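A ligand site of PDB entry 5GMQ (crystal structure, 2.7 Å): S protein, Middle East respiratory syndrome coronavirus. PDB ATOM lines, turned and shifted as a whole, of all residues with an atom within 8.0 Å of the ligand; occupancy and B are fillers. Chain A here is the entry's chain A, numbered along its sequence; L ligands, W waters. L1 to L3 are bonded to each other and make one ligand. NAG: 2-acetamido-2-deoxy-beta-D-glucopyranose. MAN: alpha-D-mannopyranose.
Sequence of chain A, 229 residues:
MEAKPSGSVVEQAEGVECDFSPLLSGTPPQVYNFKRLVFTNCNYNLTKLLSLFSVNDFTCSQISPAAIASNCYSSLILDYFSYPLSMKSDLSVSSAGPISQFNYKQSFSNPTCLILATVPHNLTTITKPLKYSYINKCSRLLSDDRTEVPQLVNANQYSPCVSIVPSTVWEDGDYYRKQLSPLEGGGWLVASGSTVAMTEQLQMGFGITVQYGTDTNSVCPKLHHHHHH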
ATOM      1  N   THR A  47     -33.322 -11.081 -32.905  1.00  0.00           N
ATOM      2  CA  THR A  47     -32.264 -12.086 -32.875  1.00  0.00           C
ATOM      3  C   THR A  47     -31.119 -11.678 -33.794  1.00  0.00           C
ATOM      4  O   THR A  47     -29.953 -11.873 -33.454  1.00  0.00           O
ATOM      5  CB  THR A  47     -32.809 -13.466 -33.265  1.00  0.00           C
ATOM      6  OG1 THR A  47     -32.985 -13.551 -34.682  1.00  0.00           O
ATOM      7  CG2 THR A  47     -34.162 -13.738 -32.562  1.00  0.00           C
ATOM      8  N   LYS A  48     -31.442 -11.086 -34.947  1.00  0.00           N
ATOM      9  CA  LYS A  48     -30.391 -10.641 -35.858  1.00  0.00           C
ATOM     10  C   LYS A  48     -29.416  -9.726 -35.152  1.00  0.00           C
ATOM     11  O   LYS A  48     -28.199  -9.846 -35.322  1.00  0.00           O
ATOM     12  CB  LYS A  48     -30.998  -9.960 -37.082  1.00  0.00           C
ATOM     13  CG  LYS A  48     -29.936  -9.441 -38.067  1.00  0.00           C
ATOM     14  CD  LYS A  48     -30.558  -8.671 -39.216  1.00  0.00           C
ATOM     15  CE  LYS A  48     -31.404  -7.516 -38.714  1.00  0.00           C
ATOM     16  NZ  LYS A  48     -30.693  -6.747 -37.637  1.00  0.00           N
ATOM     17  N   LEU A  50     -28.988  -9.434 -31.686  1.00  0.00           N
ATOM     18  CA  LEU A  50     -28.343 -10.076 -30.551  1.00  0.00           C
ATOM     19  C   LEU A  50     -27.370 -11.153 -30.982  1.00  0.00           C
ATOM     20  O   LEU A  50     -26.375 -11.393 -30.298  1.00  0.00           O
ATOM     21  CB  LEU A  50     -29.385 -10.656 -29.599  1.00  0.00           C
ATOM     22  CG  LEU A  50     -30.409  -9.650 -29.081  1.00  0.00           C
ATOM     23  CD1 LEU A  50     -31.337 -10.296 -28.096  1.00  0.00           C
ATOM     24  CD2 LEU A  50     -29.729  -8.461 -28.446  1.00  0.00           C
ATOM     25  N   SER A  51     -27.619 -11.801 -32.130  1.00  0.00           N
ATOM     26  CA  SER A  51     -26.710 -12.845 -32.602  1.00  0.00           C
ATOM     27  C   SER A  51     -25.334 -12.322 -32.957  1.00  0.00           C
ATOM     28  O   SER A  51     -24.432 -13.127 -33.201  1.00  0.00           O
ATOM     29  CB  SER A  51     -27.298 -13.538 -33.812  1.00  0.00           C
ATOM     30  OG  SER A  51     -27.129 -12.730 -34.946  1.00  0.00           O
ATOM     31  N   LEU A  52     -25.131 -11.014 -33.018  1.00  0.00           N
ATOM     32  CA  LEU A  52     -23.837 -10.437 -33.305  1.00  0.00           C
ATOM     33  C   LEU A  52     -22.951 -10.340 -32.077  1.00  0.00           C
ATOM     34  O   LEU A  52     -21.747 -10.133 -32.221  1.00  0.00           O
ATOM     35  CB  LEU A  52     -23.997  -9.050 -33.927  1.00  0.00           C
ATOM     36  CG  LEU A  52     -24.797  -8.965 -35.234  1.00  0.00           C
ATOM     37  CD1 LEU A  52     -25.012  -7.538 -35.627  1.00  0.00           C
ATOM     38  CD2 LEU A  52     -24.032  -9.648 -36.303  1.00  0.00           C
ATOM     39  N   PHE A  53     -23.507 -10.503 -30.878  1.00  0.00           N
ATOM     40  CA  PHE A  53     -22.800 -10.357 -29.619  1.00  0.00           C
ATOM     41  C   PHE A  53     -22.668 -11.723 -28.960  1.00  0.00           C
ATOM     42  O   PHE A  53     -23.173 -12.721 -29.460  1.00  0.00           O
ATOM     43  CB  PHE A  53     -23.534  -9.374 -28.702  1.00  0.00           C
ATOM     44  CG  PHE A  53     -23.661  -7.984 -29.282  1.00  0.00           C
ATOM     45  CD1 PHE A  53     -24.644  -7.694 -30.180  1.00  0.00           C
ATOM     46  CD2 PHE A  53     -22.798  -6.989 -28.894  1.00  0.00           C
ATOM     47  CE1 PHE A  53     -24.763  -6.434 -30.710  1.00  0.00           C
ATOM     48  CE2 PHE A  53     -22.916  -5.723 -29.417  1.00  0.00           C
ATOM     49  CZ  PHE A  53     -23.897  -5.452 -30.326  1.00  0.00           C
ATOM     50  N   SER A  54     -21.974 -11.763 -27.830  1.00  0.00           N
ATOM     51  CA  SER A  54     -22.035 -12.899 -26.921  1.00  0.00           C
ATOM     52  C   SER A  54     -22.882 -12.482 -25.730  1.00  0.00           C
ATOM     53  O   SER A  54     -22.406 -11.830 -24.808  1.00  0.00           O
ATOM     54  CB  SER A  54     -20.654 -13.363 -26.483  1.00  0.00           C
ATOM     55  OG  SER A  54     -20.756 -14.316 -25.452  1.00  0.00           O
ATOM     56  N   VAL A  55     -24.169 -12.840 -25.769  1.00  0.00           N
ATOM     57  CA  VAL A  55     -25.093 -12.410 -24.724  1.00  0.00           C
ATOM     58  C   VAL A  55     -24.758 -13.149 -23.450  1.00  0.00           C
ATOM     59  O   VAL A  55     -24.732 -14.378 -23.413  1.00  0.00           O
ATOM     60  CB  VAL A  55     -26.539 -12.660 -25.143  1.00  0.00           C
ATOM     61  CG1 VAL A  55     -27.463 -12.277 -24.031  1.00  0.00           C
ATOM     62  CG2 VAL A  55     -26.852 -11.886 -26.417  1.00  0.00           C
ATOM     63  N   ASN A  56     -24.495 -12.409 -22.388  1.00  0.00           N
ATOM     64  CA  ASN A  56     -24.201 -12.990 -21.095  1.00  0.00           C
ATOM     65  C   ASN A  56     -25.426 -13.106 -20.194  1.00  0.00           C
ATOM     66  O   ASN A  56     -25.576 -14.091 -19.485  1.00  0.00           O
ATOM     67  CB  ASN A  56     -23.113 -12.186 -20.409  1.00  0.00           C
ATOM     68  CG  ASN A  56     -21.855 -12.062 -21.259  1.00  0.00           C
ATOM     69  OD1 ASN A  56     -21.377 -10.976 -21.499  1.00  0.00           O
ATOM     70  ND2 ASN A  56     -21.329 -13.187 -21.717  1.00  0.00           N
ATOM     71  N   ASP A  57     -26.336 -12.134 -20.227  1.00  0.00           N
ATOM     72  CA  ASP A  57     -27.592 -12.220 -19.522  1.00  0.00           C
ATOM     73  C   ASP A  57     -28.708 -11.675 -20.396  1.00  0.00           C
ATOM     74  O   ASP A  57     -28.479 -10.920 -21.333  1.00  0.00           O
ATOM     75  CB  ASP A  57     -27.582 -11.475 -18.200  1.00  0.00           C
ATOM     76  CG  ASP A  57     -26.910 -12.236 -17.134  1.00  0.00           C
ATOM     77  OD1 ASP A  57     -27.585 -13.080 -16.497  1.00  0.00           O
ATOM     78  OD2 ASP A  57     -25.702 -12.000 -16.925  1.00  0.00           O
ATOM     79  N   PHE A  58     -29.925 -12.060 -20.062  1.00  0.00           N
ATOM     80  CA  PHE A  58     -31.081 -11.677 -20.862  1.00  0.00           C
ATOM     81  C   PHE A  58     -32.284 -11.915 -19.931  1.00  0.00           C
ATOM     82  O   PHE A  58     -32.809 -13.011 -19.836  1.00  0.00           O
ATOM     83  CB  PHE A  58     -31.160 -12.478 -22.141  1.00  0.00           C
ATOM     84  CG  PHE A  58     -32.147 -11.970 -23.134  1.00  0.00           C
ATOM     85  CD1 PHE A  58     -33.128 -11.084 -22.780  1.00  0.00           C
ATOM     86  CD2 PHE A  58     -32.109 -12.412 -24.430  1.00  0.00           C
ATOM     87  CE1 PHE A  58     -34.036 -10.642 -23.713  1.00  0.00           C
ATOM     88  CE2 PHE A  58     -33.004 -11.975 -25.361  1.00  0.00           C
ATOM     89  CZ  PHE A  58     -33.963 -11.086 -24.999  1.00  0.00           C
ATOM     90  N   LEU A  85     -19.897  -6.339 -16.888  1.00  0.00           N
ATOM     91  CA  LEU A  85     -20.615  -7.507 -16.394  1.00  0.00           C
ATOM     92  C   LEU A  85     -20.514  -7.670 -14.892  1.00  0.00           C
ATOM     93  O   LEU A  85     -21.449  -8.139 -14.250  1.00  0.00           O
ATOM     94  CB  LEU A  85     -20.079  -8.768 -17.039  1.00  0.00           C
ATOM     95  CG  LEU A  85     -21.033  -9.605 -17.858  1.00  0.00           C
ATOM     96  CD1 LEU A  85     -22.217  -9.988 -17.013  1.00  0.00           C
ATOM     97  CD2 LEU A  85     -21.435  -8.780 -19.086  1.00  0.00           C
ATOM     98  N   LYS A  88     -23.511  -6.394 -13.001  1.00  0.00           N
ATOM     99  CA  LYS A  88     -24.830  -6.922 -13.332  1.00  0.00           C
ATOM    100  C   LYS A  88     -25.829  -6.772 -12.193  1.00  0.00           C
ATOM    101  O   LYS A  88     -26.966  -6.372 -12.406  1.00  0.00           O
ATOM    102  CB  LYS A  88     -24.704  -8.376 -13.755  1.00  0.00           C
ATOM    103  CG  LYS A  88     -25.856  -9.301 -13.443  1.00  0.00           C
ATOM    104  CD  LYS A  88     -25.500 -10.742 -13.834  1.00  0.00           C
ATOM    105  CE  LYS A  88     -26.154 -11.758 -12.918  1.00  0.00           C
ATOM    106  NZ  LYS A  88     -25.422 -13.061 -12.940  1.00  0.00           N
ATOM    107  N   LEU A 116     -27.177  -7.987 -21.045  1.00  0.00           N
ATOM    108  CA  LEU A 116     -25.762  -7.704 -20.897  1.00  0.00           C
ATOM    109  C   LEU A 116     -25.020  -8.568 -21.893  1.00  0.00           C
ATOM    110  O   LEU A 116     -25.241  -9.776 -21.943  1.00  0.00           O
ATOM    111  CB  LEU A 116     -25.297  -7.975 -19.475  1.00  0.00           C
ATOM    112  CG  LEU A 116     -26.186  -7.354 -18.415  1.00  0.00           C
ATOM    113  CD1 LEU A 116     -25.539  -7.480 -17.080  1.00  0.00           C
ATOM    114  CD2 LEU A 116     -26.484  -5.905 -18.730  1.00  0.00           C
ATOM    115  N   ALA A 117     -24.162  -7.954 -22.694  1.00  0.00           N
ATOM    116  CA  ALA A 117     -23.516  -8.657 -23.787  1.00  0.00           C
ATOM    117  C   ALA A 117     -22.059  -8.249 -23.857  1.00  0.00           C
ATOM    118  O   ALA A 117     -21.662  -7.209 -23.352  1.00  0.00           O
ATOM    119  CB  ALA A 117     -24.218  -8.380 -25.122  1.00  0.00           C
ATOM    120  N   THR A 118     -21.262  -9.112 -24.463  1.00  0.00           N
ATOM    121  CA  THR A 118     -19.831  -8.930 -24.633  1.00  0.00           C
ATOM    122  C   THR A 118     -19.578  -8.825 -26.128  1.00  0.00           C
ATOM    123  O   THR A 118     -20.170  -9.569 -26.907  1.00  0.00           O
ATOM    124  CB  THR A 118     -19.036 -10.105 -24.025  1.00  0.00           C
ATOM    125  OG1 THR A 118     -19.273 -10.174 -22.627  1.00  0.00           O
ATOM    126  CG2 THR A 118     -17.562  -9.937 -24.250  1.00  0.00           C
ATOM    127  N   PRO A 120     -17.670  -9.423 -29.355  1.00  0.00           N
ATOM    128  CA  PRO A 120     -16.636 -10.296 -29.890  1.00  0.00           C
ATOM    129  C   PRO A 120     -15.659  -9.544 -30.780  1.00  0.00           C
ATOM    130  O   PRO A 120     -15.849  -8.377 -31.123  1.00  0.00           O
ATOM    131  CB  PRO A 120     -17.447 -11.307 -30.691  1.00  0.00           C
ATOM    132  CG  PRO A 120     -18.620 -10.552 -31.122  1.00  0.00           C
ATOM    133  CD  PRO A 120     -18.960  -9.654 -30.004  1.00  0.00           C
ATOM    134  N   ASN A 122     -14.638  -9.974 -34.029  1.00  0.00           N
ATOM    135  CA  ASN A 122     -15.068  -9.561 -35.368  1.00  0.00           C
ATOM    136  C   ASN A 122     -16.021  -8.382 -35.341  1.00  0.00           C
ATOM    137  O   ASN A 122     -16.364  -7.862 -36.410  1.00  0.00           O
ATOM    138  CB  ASN A 122     -15.750 -10.706 -36.116  1.00  0.00           C
ATOM    139  CG  ASN A 122     -16.410 -11.653 -35.185  1.00  0.00           C
ATOM    140  OD1 ASN A 122     -15.990 -11.735 -34.039  1.00  0.00           O
ATOM    141  ND2 ASN A 122     -17.444 -12.396 -35.651  1.00  0.00           N
ATOM    142  N   GLN A 201     -12.609  -7.241 -23.846  1.00  0.00           N
ATOM    143  CA  GLN A 201     -13.646  -6.982 -24.815  1.00  0.00           C
ATOM    144  C   GLN A 201     -14.703  -6.082 -24.176  1.00  0.00           C
ATOM    145  O   GLN A 201     -14.994  -6.205 -22.990  1.00  0.00           O
ATOM    146  CB  GLN A 201     -14.273  -8.281 -25.298  1.00  0.00           C
ATOM    147  CG  GLN A 201     -13.241  -9.374 -25.532  1.00  0.00           C
ATOM    148  CD  GLN A 201     -13.859 -10.608 -26.144  1.00  0.00           C
ATOM    149  OE1 GLN A 201     -14.272 -10.584 -27.288  1.00  0.00           O
ATOM    150  NE2 GLN A 201     -13.929 -11.696 -25.374  1.00  0.00           N
ATOM    151  N   GLN A 203     -17.976  -4.640 -22.791  1.00  0.00           N
ATOM    152  CA  GLN A 203     -19.205  -5.193 -22.249  1.00  0.00           C
ATOM    153  C   GLN A 203     -20.293  -4.134 -22.251  1.00  0.00           C
ATOM    154  O   GLN A 203     -20.102  -3.039 -21.728  1.00  0.00           O
ATOM    155  CB  GLN A 203     -18.978  -5.742 -20.851  1.00  0.00           C
ATOM    156  CG  GLN A 203     -18.149  -6.989 -20.895  1.00  0.00           C
ATOM    157  CD  GLN A 203     -17.787  -7.569 -19.549  1.00  0.00           C
ATOM    158  OE1 GLN A 203     -17.738  -6.879 -18.531  1.00  0.00           O
ATOM    159  NE2 GLN A 203     -17.524  -8.852 -19.532  1.00  0.00           N
HETATM  160  C1  NAG L   1     -21.355 -15.370 -31.763  1.00  0.00           C
HETATM  161  C2  NAG L   1     -22.572 -16.258 -31.914  1.00  0.00           C
HETATM  162  C3  NAG L   1     -23.384 -16.264 -30.616  1.00  0.00           C
HETATM  163  C4  NAG L   1     -22.516 -16.655 -29.426  1.00  0.00           C
HETATM  164  C5  NAG L   1     -21.212 -15.856 -29.403  1.00  0.00           C
HETATM  165  C6  NAG L   1     -20.217 -16.417 -28.400  1.00  0.00           C
HETATM  166  C7  NAG L   1     -23.592 -16.635 -34.110  1.00  0.00           C
HETATM  167  C8  NAG L   1     -24.457 -16.071 -35.186  1.00  0.00           C
HETATM  168  N2  NAG L   1     -23.392 -15.858 -33.042  1.00  0.00           N
HETATM  169  O3  NAG L   1     -24.451 -17.193 -30.741  1.00  0.00           O
HETATM  170  O4  NAG L   1     -23.148 -16.286 -28.210  1.00  0.00           O
HETATM  171  O5  NAG L   1     -20.557 -15.846 -30.678  1.00  0.00           O
HETATM  172  O6  NAG L   1     -18.984 -16.749 -29.008  1.00  0.00           O
HETATM  173  O7  NAG L   1     -23.096 -17.749 -34.200  1.00  0.00           O
HETATM  174  C1  MAN L   2     -24.056 -17.207 -27.562  1.00  0.00           C
HETATM  175  C2  MAN L   2     -23.706 -17.109 -26.049  1.00  0.00           C
HETATM  176  C3  MAN L   2     -23.722 -18.530 -25.473  1.00  0.00           C
HETATM  177  C4  MAN L   2     -24.975 -19.270 -25.910  1.00  0.00           C
HETATM  178  C5  MAN L   2     -24.958 -19.469 -27.413  1.00  0.00           C
HETATM  179  C6  MAN L   2     -26.310 -19.211 -28.042  1.00  0.00           C
HETATM  180  O2  MAN L   2     -24.696 -16.370 -25.417  1.00  0.00           O
HETATM  181  O3  MAN L   2     -23.517 -18.717 -24.047  1.00  0.00           O
HETATM  182  O4  MAN L   2     -24.994 -20.525 -25.287  1.00  0.00           O
HETATM  183  O5  MAN L   2     -23.979 -18.561 -28.011  1.00  0.00           O
HETATM  184  O6  MAN L   2     -26.416 -19.936 -29.260  1.00  0.00           O
HETATM  185  C1  MAN L   3     -23.161 -17.637 -23.181  1.00  0.00           C
HETATM  186  C2  MAN L   3     -21.714 -17.824 -22.486  1.00  0.00           C
HETATM  187  C3  MAN L   3     -21.576 -16.934 -21.211  1.00  0.00           C
HETATM  188  C4  MAN L   3     -22.952 -16.620 -20.627  1.00  0.00           C
HETATM  189  C5  MAN L   3     -23.739 -17.835 -20.937  1.00  0.00           C
HETATM  190  C6  MAN L   3     -24.869 -18.148 -20.058  1.00  0.00           C
HETATM  191  O2  MAN L   3     -20.536 -17.534 -23.294  1.00  0.00           O
HETATM  192  O3  MAN L   3     -20.879 -15.772 -21.472  1.00  0.00           O
HETATM  193  O4  MAN L   3     -22.895 -16.393 -19.258  1.00  0.00           O
HETATM  194  O5  MAN L   3     -24.182 -17.584 -22.263  1.00  0.00           O
HETATM  195  O6  MAN L   3     -24.939 -19.592 -20.050  1.00  0.00           O
HETATM  196  O   HOH W   1     -29.230 -18.769 -28.645  1.00  0.00           O
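ND2 of Asn 56 is in hydrogen-bond range of O3 of MAN L3, at 2.6 Å. O2 of MAN L2 sits at hydrogen-bond distance from O of Val 55, 2.8 Å away. A nitrogen (N2) of NAG L1 is in hydrogen-bond range of the backbone carbonyl oxygen (O) of Ser 51, at 2.9 Å.
OD1 of Asn 56 sits at hydrogen-bond distance from OG1 of Thr 118 (2.5 Å). The backbone NH of Asn 56 is in hydrogen-bond range of the backbone carbonyl oxygen of Leu 116, 2.8 Å away. The backbone carbonyl oxygen (O) of Thr 47 lies close to the side-chain hydroxyl (OG) of Ser 51 (3.3 Å). The backbone carbonyl oxygen of Lys 48 sits at hydrogen-bond distance from the side-chain hydroxyl of Ser 51. The backbone carbonyl oxygen (O) of Ser 54 sits at hydrogen-bond distance from the backbone NH (N) of Thr 118 (3.0 Å).
Phe 53 touches the ligand. CB of Ser 54 touches C6 of NAG L1, at 3.6 Å. Within 4 Å of the ligand: Ser 51, Phe 53, Ser 54, Val 55 and Asn 56. The nearest printed residue that does not touch the ligand is Leu 52 (5.1 Å).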
